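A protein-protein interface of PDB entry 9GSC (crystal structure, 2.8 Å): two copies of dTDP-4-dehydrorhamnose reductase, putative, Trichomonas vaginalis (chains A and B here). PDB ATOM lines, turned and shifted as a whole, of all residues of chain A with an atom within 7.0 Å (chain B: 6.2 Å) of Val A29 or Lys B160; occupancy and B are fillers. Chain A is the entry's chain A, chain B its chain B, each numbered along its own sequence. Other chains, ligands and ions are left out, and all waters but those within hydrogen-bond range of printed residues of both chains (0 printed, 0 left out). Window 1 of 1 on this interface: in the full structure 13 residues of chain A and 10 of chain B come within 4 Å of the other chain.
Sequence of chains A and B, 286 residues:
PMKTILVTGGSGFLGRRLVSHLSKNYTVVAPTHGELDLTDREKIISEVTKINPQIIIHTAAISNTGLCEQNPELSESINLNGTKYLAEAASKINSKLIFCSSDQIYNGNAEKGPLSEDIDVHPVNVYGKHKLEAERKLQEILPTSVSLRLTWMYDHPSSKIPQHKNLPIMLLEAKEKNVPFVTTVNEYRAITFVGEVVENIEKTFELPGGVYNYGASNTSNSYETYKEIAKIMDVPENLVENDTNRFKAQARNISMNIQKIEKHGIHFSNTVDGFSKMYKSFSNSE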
ATOM      1  N   MET A   2      10.962 -20.909  11.649  1.00  0.00           N
ATOM      2  CA  MET A   2      10.536 -21.754  10.538  1.00  0.00           C
ATOM      3  C   MET A   2       9.078 -21.544  10.157  1.00  0.00           C
ATOM      4  O   MET A   2       8.184 -21.646  10.998  1.00  0.00           O
ATOM      5  CB  MET A   2      10.752 -23.232  10.859  1.00  0.00           C
ATOM      6  CG  MET A   2      12.019 -23.819  10.274  1.00  0.00           C
ATOM      7  SD  MET A   2      11.961 -25.619  10.260  1.00  0.00           S
ATOM      8  CE  MET A   2      13.585 -26.006   9.612  1.00  0.00           C
ATOM      9  N   LYS A   3       8.854 -21.201   8.893  1.00  0.00           N
ATOM     10  CA  LYS A   3       7.503 -20.931   8.424  1.00  0.00           C
ATOM     11  C   LYS A   3       6.665 -22.207   8.403  1.00  0.00           C
ATOM     12  O   LYS A   3       7.160 -23.289   8.080  1.00  0.00           O
ATOM     13  CB  LYS A   3       7.534 -20.288   7.036  1.00  0.00           C
ATOM     14  CG  LYS A   3       7.958 -18.822   7.055  1.00  0.00           C
ATOM     15  CD  LYS A   3       7.819 -18.166   5.686  1.00  0.00           C
ATOM     16  CE  LYS A   3       6.477 -17.464   5.536  1.00  0.00           C
ATOM     17  NZ  LYS A   3       6.442 -16.572   4.344  1.00  0.00           N
ATOM     18  N   THR A   4       5.389 -22.074   8.761  1.00  0.00           N
ATOM     19  CA  THR A   4       4.483 -23.207   8.905  1.00  0.00           C
ATOM     20  C   THR A   4       3.586 -23.266   7.675  1.00  0.00           C
ATOM     21  O   THR A   4       3.044 -22.240   7.250  1.00  0.00           O
ATOM     22  CB  THR A   4       3.637 -23.085  10.175  1.00  0.00           C
ATOM     23  OG1 THR A   4       4.495 -22.982  11.318  1.00  0.00           O
ATOM     24  CG2 THR A   4       2.733 -24.302  10.335  1.00  0.00           C
ATOM     25  N   ILE A   5       3.419 -24.462   7.116  1.00  0.00           N
ATOM     26  CA  ILE A   5       2.669 -24.646   5.880  1.00  0.00           C
ATOM     27  C   ILE A   5       1.586 -25.693   6.100  1.00  0.00           C
ATOM     28  O   ILE A   5       1.848 -26.756   6.675  1.00  0.00           O
ATOM     29  CB  ILE A   5       3.596 -25.055   4.719  1.00  0.00           C
ATOM     30  CG1 ILE A   5       4.351 -23.833   4.199  1.00  0.00           C
ATOM     31  CG2 ILE A   5       2.813 -25.716   3.596  1.00  0.00           C
ATOM     32  CD1 ILE A   5       5.359 -24.155   3.129  1.00  0.00           C
ATOM     33  N   LEU A   6       0.378 -25.395   5.626  1.00  0.00           N
ATOM     34  CA  LEU A   6      -0.749 -26.317   5.660  1.00  0.00           C
ATOM     35  C   LEU A   6      -0.939 -26.926   4.277  1.00  0.00           C
ATOM     36  O   LEU A   6      -1.095 -26.199   3.290  1.00  0.00           O
ATOM     37  CB  LEU A   6      -2.015 -25.586   6.105  1.00  0.00           C
ATOM     38  CG  LEU A   6      -3.404 -26.210   6.007  1.00  0.00           C
ATOM     39  CD1 LEU A   6      -3.400 -27.564   6.640  1.00  0.00           C
ATOM     40  CD2 LEU A   6      -4.423 -25.315   6.692  1.00  0.00           C
ATOM     41  N   VAL A   7      -0.931 -28.254   4.208  1.00  0.00           N
ATOM     42  CA  VAL A   7      -1.148 -28.987   2.967  1.00  0.00           C
ATOM     43  C   VAL A   7      -2.416 -29.814   3.127  1.00  0.00           C
ATOM     44  O   VAL A   7      -2.493 -30.675   4.013  1.00  0.00           O
ATOM     45  CB  VAL A   7       0.051 -29.884   2.616  1.00  0.00           C
ATOM     46  CG1 VAL A   7      -0.080 -30.416   1.199  1.00  0.00           C
ATOM     47  CG2 VAL A   7       1.354 -29.120   2.788  1.00  0.00           C
ATOM     48  N   THR A   8      -3.405 -29.558   2.274  1.00  0.00           N
ATOM     49  CA  THR A   8      -4.629 -30.346   2.267  1.00  0.00           C
ATOM     50  C   THR A   8      -4.444 -31.575   1.388  1.00  0.00           C
ATOM     51  O   THR A   8      -3.768 -31.521   0.356  1.00  0.00           O
ATOM     52  CB  THR A   8      -5.817 -29.521   1.768  1.00  0.00           C
ATOM     53  OG1 THR A   8      -5.607 -29.151   0.402  1.00  0.00           O
ATOM     54  CG2 THR A   8      -5.986 -28.266   2.610  1.00  0.00           C
ATOM     55  N   VAL A  19       4.478 -32.804   1.278  1.00  0.00           N
ATOM     56  CA  VAL A  19       4.757 -32.811   2.710  1.00  0.00           C
ATOM     57  C   VAL A  19       6.146 -33.381   2.966  1.00  0.00           C
ATOM     58  O   VAL A  19       6.939 -32.817   3.727  1.00  0.00           O
ATOM     59  CB  VAL A  19       3.673 -33.601   3.466  1.00  0.00           C
ATOM     60  CG1 VAL A  19       4.091 -33.838   4.914  1.00  0.00           C
ATOM     61  CG2 VAL A  19       2.342 -32.869   3.398  1.00  0.00           C
ATOM     62  N   THR A  27       7.813 -26.394   8.705  1.00  0.00           N
ATOM     63  CA  THR A  27       6.913 -27.088   9.627  1.00  0.00           C
ATOM     64  C   THR A  27       5.618 -27.358   8.866  1.00  0.00           C
ATOM     65  O   THR A  27       4.805 -26.452   8.663  1.00  0.00           O
ATOM     66  CB  THR A  27       6.663 -26.252  10.880  1.00  0.00           C
ATOM     67  OG1 THR A  27       7.903 -25.715  11.356  1.00  0.00           O
ATOM     68  CG2 THR A  27       6.029 -27.097  11.976  1.00  0.00           C
ATOM     69  N   VAL A  28       5.424 -28.607   8.451  1.00  0.00           N
ATOM     70  CA  VAL A  28       4.294 -28.994   7.611  1.00  0.00           C
ATOM     71  C   VAL A  28       3.207 -29.640   8.460  1.00  0.00           C
ATOM     72  O   VAL A  28       3.467 -30.602   9.194  1.00  0.00           O
ATOM     73  CB  VAL A  28       4.746 -29.938   6.484  1.00  0.00           C
ATOM     74  CG1 VAL A  28       3.573 -30.278   5.587  1.00  0.00           C
ATOM     75  CG2 VAL A  28       5.863 -29.293   5.688  1.00  0.00           C
ATOM     76  N   VAL A  29       1.988 -29.116   8.350  1.00  0.00           N
ATOM     77  CA  VAL A  29       0.807 -29.655   9.019  1.00  0.00           C
ATOM     78  C   VAL A  29      -0.112 -30.227   7.946  1.00  0.00           C
ATOM     79  O   VAL A  29      -0.668 -29.479   7.134  1.00  0.00           O
ATOM     80  CB  VAL A  29       0.085 -28.584   9.848  1.00  0.00           C
ATOM     81  CG1 VAL A  29      -1.024 -29.212  10.681  1.00  0.00           C
ATOM     82  CG2 VAL A  29       1.074 -27.836  10.731  1.00  0.00           C
ATOM     83  N   ALA A  30      -0.264 -31.556   7.923  1.00  0.00           N
ATOM     84  CA  ALA A  30      -1.057 -32.252   6.909  1.00  0.00           C
ATOM     85  C   ALA A  30      -2.243 -32.953   7.566  1.00  0.00           C
ATOM     86  O   ALA A  30      -2.198 -34.166   7.819  1.00  0.00           O
ATOM     87  CB  ALA A  30      -0.203 -33.251   6.130  1.00  0.00           C
ATOM     88  N   PRO A  31      -3.322 -32.224   7.852  1.00  0.00           N
ATOM     89  CA  PRO A  31      -4.505 -32.853   8.445  1.00  0.00           C
ATOM     90  C   PRO A  31      -5.145 -33.849   7.490  1.00  0.00           C
ATOM     91  O   PRO A  31      -5.010 -33.764   6.267  1.00  0.00           O
ATOM     92  CB  PRO A  31      -5.435 -31.666   8.724  1.00  0.00           C
ATOM     93  CG  PRO A  31      -4.993 -30.624   7.752  1.00  0.00           C
ATOM     94  CD  PRO A  31      -3.502 -30.774   7.707  1.00  0.00           C
ATOM     95  N   GLU A  47      -9.465 -24.460  12.747  1.00  0.00           N
ATOM     96  CA  GLU A  47      -8.162 -25.092  12.545  1.00  0.00           C
ATOM     97  C   GLU A  47      -7.196 -24.137  11.855  1.00  0.00           C
ATOM     98  O   GLU A  47      -6.070 -23.936  12.321  1.00  0.00           O
ATOM     99  CB  GLU A  47      -8.309 -26.401  11.767  1.00  0.00           C
ATOM    100  CG  GLU A  47      -8.940 -27.540  12.577  1.00  0.00           C
ATOM    101  CD  GLU A  47      -7.984 -28.178  13.581  1.00  0.00           C
ATOM    102  OE1 GLU A  47      -7.630 -27.517  14.581  1.00  0.00           O
ATOM    103  OE2 GLU A  47      -7.597 -29.349  13.378  1.00  0.00           O
ATOM    104  N   LYS A  50      -6.325 -21.742  14.399  1.00  0.00           N
ATOM    105  CA  LYS A  50      -5.427 -22.313  15.402  1.00  0.00           C
ATOM    106  C   LYS A  50      -4.069 -22.673  14.806  1.00  0.00           C
ATOM    107  O   LYS A  50      -3.026 -22.308  15.360  1.00  0.00           O
ATOM    108  CB  LYS A  50      -6.051 -23.556  16.046  1.00  0.00           C
ATOM    109  CG  LYS A  50      -7.461 -23.401  16.604  1.00  0.00           C
ATOM    110  CD  LYS A  50      -7.614 -22.178  17.481  1.00  0.00           C
ATOM    111  CE  LYS A  50      -8.770 -22.362  18.451  1.00  0.00           C
ATOM    112  NZ  LYS A  50      -8.320 -22.958  19.738  1.00  0.00           N
ATOM    113  N   ILE A  51      -4.057 -23.392  13.680  1.00  0.00           N
ATOM    114  CA  ILE A  51      -2.789 -23.757  13.046  1.00  0.00           C
ATOM    115  C   ILE A  51      -1.972 -22.520  12.683  1.00  0.00           C
ATOM    116  O   ILE A  51      -0.759 -22.477  12.918  1.00  0.00           O
ATOM    117  CB  ILE A  51      -3.028 -24.664  11.823  1.00  0.00           C
ATOM    118  CG1 ILE A  51      -3.737 -25.951  12.247  1.00  0.00           C
ATOM    119  CG2 ILE A  51      -1.707 -25.031  11.178  1.00  0.00           C
ATOM    120  CD1 ILE A  51      -4.013 -26.904  11.104  1.00  0.00           C
ATOM    121  N   ASN A  52      -2.613 -21.500  12.103  1.00  0.00           N
ATOM    122  CA  ASN A  52      -1.918 -20.307  11.617  1.00  0.00           C
ATOM    123  C   ASN A  52      -0.823 -20.697  10.625  1.00  0.00           C
ATOM    124  O   ASN A  52       0.368 -20.529  10.917  1.00  0.00           O
ATOM    125  CB  ASN A  52      -1.337 -19.503  12.794  1.00  0.00           C
ATOM    126  CG  ASN A  52      -0.505 -18.285  12.356  1.00  0.00           C
ATOM    127  OD1 ASN A  52      -0.438 -17.936  11.176  1.00  0.00           O
ATOM    128  ND2 ASN A  52       0.152 -17.654  13.323  1.00  0.00           N
ATOM    129  N   PRO A  53      -1.165 -21.308   9.491  1.00  0.00           N
ATOM    130  CA  PRO A  53      -0.146 -21.556   8.464  1.00  0.00           C
ATOM    131  C   PRO A  53       0.196 -20.251   7.760  1.00  0.00           C
ATOM    132  O   PRO A  53      -0.702 -19.499   7.374  1.00  0.00           O
ATOM    133  CB  PRO A  53      -0.836 -22.542   7.512  1.00  0.00           C
ATOM    134  CG  PRO A  53      -2.027 -23.054   8.300  1.00  0.00           C
ATOM    135  CD  PRO A  53      -2.460 -21.872   9.080  1.00  0.00           C
ATOM    136  N   GLN A  54       1.492 -19.975   7.582  1.00  0.00           N
ATOM    137  CA  GLN A  54       1.809 -18.808   6.767  1.00  0.00           C
ATOM    138  C   GLN A  54       1.542 -19.080   5.293  1.00  0.00           C
ATOM    139  O   GLN A  54       1.338 -18.133   4.527  1.00  0.00           O
ATOM    140  CB  GLN A  54       3.266 -18.332   6.915  1.00  0.00           C
ATOM    141  CG  GLN A  54       3.666 -17.641   8.229  1.00  0.00           C
ATOM    142  CD  GLN A  54       3.975 -18.597   9.361  1.00  0.00           C
ATOM    143  OE1 GLN A  54       3.296 -18.633  10.383  1.00  0.00           O
ATOM    144  NE2 GLN A  54       5.078 -19.304   9.220  1.00  0.00           N
ATOM    145  N   ARG B  16       2.746 -39.967  12.386  1.00  0.00           N
ATOM    146  CA  ARG B  16       3.017 -38.644  11.822  1.00  0.00           C
ATOM    147  C   ARG B  16       4.183 -37.976  12.543  1.00  0.00           C
ATOM    148  O   ARG B  16       5.054 -37.369  11.929  1.00  0.00           O
ATOM    149  CB  ARG B  16       1.754 -37.768  11.852  1.00  0.00           C
ATOM    150  CG  ARG B  16       1.175 -37.499  13.209  1.00  0.00           C
ATOM    151  CD  ARG B  16       0.001 -36.538  13.149  1.00  0.00           C
ATOM    152  NE  ARG B  16      -1.028 -37.003  12.223  1.00  0.00           N
ATOM    153  CZ  ARG B  16      -1.842 -36.200  11.546  1.00  0.00           C
ATOM    154  NH1 ARG B  16      -2.752 -36.709  10.724  1.00  0.00           N
ATOM    155  NH2 ARG B  16      -1.738 -34.885  11.678  1.00  0.00           N
ATOM    156  N   ASP B 155       1.119 -34.529  23.103  1.00  0.00           N
ATOM    157  CA  ASP B 155       1.773 -33.389  22.489  1.00  0.00           C
ATOM    158  C   ASP B 155       1.357 -32.159  23.283  1.00  0.00           C
ATOM    159  O   ASP B 155       0.594 -32.258  24.249  1.00  0.00           O
ATOM    160  CB  ASP B 155       1.390 -33.286  21.008  1.00  0.00           C
ATOM    161  CG  ASP B 155       2.315 -32.375  20.219  1.00  0.00           C
ATOM    162  OD1 ASP B 155       3.255 -31.808  20.816  1.00  0.00           O
ATOM    163  OD2 ASP B 155       2.101 -32.227  18.996  1.00  0.00           O
ATOM    164  N   HIS B 156       1.863 -30.997  22.893  1.00  0.00           N
ATOM    165  CA  HIS B 156       1.486 -29.796  23.618  1.00  0.00           C
ATOM    166  C   HIS B 156      -0.018 -29.577  23.500  1.00  0.00           C
ATOM    167  O   HIS B 156      -0.592 -29.791  22.426  1.00  0.00           O
ATOM    168  CB  HIS B 156       2.242 -28.564  23.127  1.00  0.00           C
ATOM    169  CG  HIS B 156       2.212 -27.429  24.102  1.00  0.00           C
ATOM    170  ND1 HIS B 156       1.222 -26.470  24.096  1.00  0.00           N
ATOM    171  CD2 HIS B 156       3.024 -27.124  25.143  1.00  0.00           C
ATOM    172  CE1 HIS B 156       1.437 -25.610  25.075  1.00  0.00           C
ATOM    173  NE2 HIS B 156       2.525 -25.985  25.726  1.00  0.00           N
ATOM    174  N   SER B 158      -1.718 -26.981  23.079  1.00  0.00           N
ATOM    175  CA  SER B 158      -2.002 -26.099  21.955  1.00  0.00           C
ATOM    176  C   SER B 158      -1.030 -26.331  20.802  1.00  0.00           C
ATOM    177  O   SER B 158      -0.483 -25.374  20.245  1.00  0.00           O
ATOM    178  CB  SER B 158      -1.954 -24.637  22.402  1.00  0.00           C
ATOM    179  OG  SER B 158      -1.913 -23.769  21.284  1.00  0.00           O
ATOM    180  N   SER B 159      -0.813 -27.590  20.434  1.00  0.00           N
ATOM    181  CA  SER B 159       0.099 -27.911  19.347  1.00  0.00           C
ATOM    182  C   SER B 159      -0.593 -27.750  18.000  1.00  0.00           C
ATOM    183  O   SER B 159      -1.805 -27.945  17.872  1.00  0.00           O
ATOM    184  CB  SER B 159       0.631 -29.338  19.487  1.00  0.00           C
ATOM    185  OG  SER B 159       1.496 -29.669  18.414  1.00  0.00           O
ATOM    186  N   LYS B 160       0.195 -27.390  16.985  1.00  0.00           N
ATOM    187  CA  LYS B 160      -0.345 -27.230  15.641  1.00  0.00           C
ATOM    188  C   LYS B 160      -0.637 -28.559  14.959  1.00  0.00           C
ATOM    189  O   LYS B 160      -1.353 -28.572  13.953  1.00  0.00           O
ATOM    190  CB  LYS B 160       0.614 -26.416  14.771  1.00  0.00           C
ATOM    191  CG  LYS B 160       0.723 -24.958  15.167  1.00  0.00           C
ATOM    192  CD  LYS B 160       1.612 -24.196  14.200  1.00  0.00           C
ATOM    193  CE  LYS B 160       1.806 -22.757  14.648  1.00  0.00           C
ATOM    194  NZ  LYS B 160       2.716 -22.019  13.734  1.00  0.00           N
ATOM    195  N   ILE B 161      -0.116 -29.667  15.475  1.00  0.00           N
ATOM    196  CA  ILE B 161      -0.358 -30.961  14.848  1.00  0.00           C
ATOM    197  C   ILE B 161      -1.556 -31.595  15.544  1.00  0.00           C
ATOM    198  O   ILE B 161      -1.615 -31.617  16.782  1.00  0.00           O
ATOM    199  CB  ILE B 161       0.882 -31.866  14.925  1.00  0.00           C
ATOM    200  CG1 ILE B 161       2.122 -31.123  14.423  1.00  0.00           C
ATOM    201  CG2 ILE B 161       0.675 -33.134  14.115  1.00  0.00           C
ATOM    202  CD1 ILE B 161       3.426 -31.781  14.820  1.00  0.00           C
ATOM    203  N   PRO B 162      -2.534 -32.101  14.793  1.00  0.00           N
ATOM    204  CA  PRO B 162      -3.737 -32.657  15.417  1.00  0.00           C
ATOM    205  C   PRO B 162      -3.417 -33.854  16.297  1.00  0.00           C
ATOM    206  O   PRO B 162      -2.477 -34.610  16.044  1.00  0.00           O
ATOM    207  CB  PRO B 162      -4.601 -33.058  14.216  1.00  0.00           C
ATOM    208  CG  PRO B 162      -4.156 -32.125  13.139  1.00  0.00           C
ATOM    209  CD  PRO B 162      -2.665 -32.060  13.327  1.00  0.00           C
ATOM    210  N   PHE B 282       7.146 -24.028  24.286  1.00  0.00           N
ATOM    211  CA  PHE B 282       6.049 -23.226  23.751  1.00  0.00           C
ATOM    212  C   PHE B 282       5.958 -21.877  24.450  1.00  0.00           C
ATOM    213  O   PHE B 282       5.045 -21.648  25.238  1.00  0.00           O
ATOM    214  CB  PHE B 282       4.715 -23.961  23.894  1.00  0.00           C
ATOM    215  CG  PHE B 282       4.180 -24.538  22.619  1.00  0.00           C
ATOM    216  CD1 PHE B 282       3.108 -23.935  21.986  1.00  0.00           C
ATOM    217  CD2 PHE B 282       4.748 -25.663  22.038  1.00  0.00           C
ATOM    218  CE1 PHE B 282       2.594 -24.433  20.811  1.00  0.00           C
ATOM    219  CE2 PHE B 282       4.234 -26.171  20.849  1.00  0.00           C
ATOM    220  CZ  PHE B 282       3.157 -25.553  20.239  1.00  0.00           C
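N of Gln A54 sits at hydrogen-bond distance from O of Thr A4 (2.8 Å).
The backbone NH (N) of Val A7 is in hydrogen-bond range of the backbone carbonyl oxygen (O) of Val A29 (3.2 Å).
The backbone NH of Val A29 is in hydrogen-bond range of the backbone carbonyl oxygen of Ile A5, at 2.9 Å.
Of chain B, only Lys B160 (3.4 Å) comes within 4 Å of Val A29.
Of chain A, only Thr A4, Val A29, Ile A51 and Asn A52 come within 4 Å of Lys B160.
Printed residues of chain B within 4 Å of Ala A30: Arg B16 (3.9 Å).
Printed residues of chain B within 4 Å of Asn A52: Lys B160.
Of the printed residues of chain A, Arg B16 touches Ala A30 (3.9 Å).
Printed residues of chain B within 4 Å of Ile A51: Lys B160.
The nearest residue of chain B that does not touch Val A29 is Pro B162 (4.2 Å).
The nearest residue of chain A that does not touch Lys B160 is Lys A50 (4.6 Å).
The nearest printed residue of chain B that does not touch Ile A51 is Pro B162 (5.6 Å).
Val A29 touches Lys B160 (CG1 to O, 3.4 Å).
Ala A30 touches Arg B16 (O to NH1, 3.9 Å).
Lys B160 touches Ile A51 (CE to O, 3.1 Å).
O of Asn A52 touches NZ of Lys B160, at 3.96 Å.
No position is printed for both chains.
Of the 5 pairs that touch across the chains among the printed residues, none has its exchanged pair printed and touching as well.
NZ of Lys B160 lies within hydrogen-bond range of OG1 of Thr A4 (3.2 Å).
Of the 9 printed residues of chain B, 2 touch a printed residue of chain A.
Among the printed residues, no Asp or Glu carboxylate lies within 4 Å of a Lys or Arg side-chain nitrogen of the other chain.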
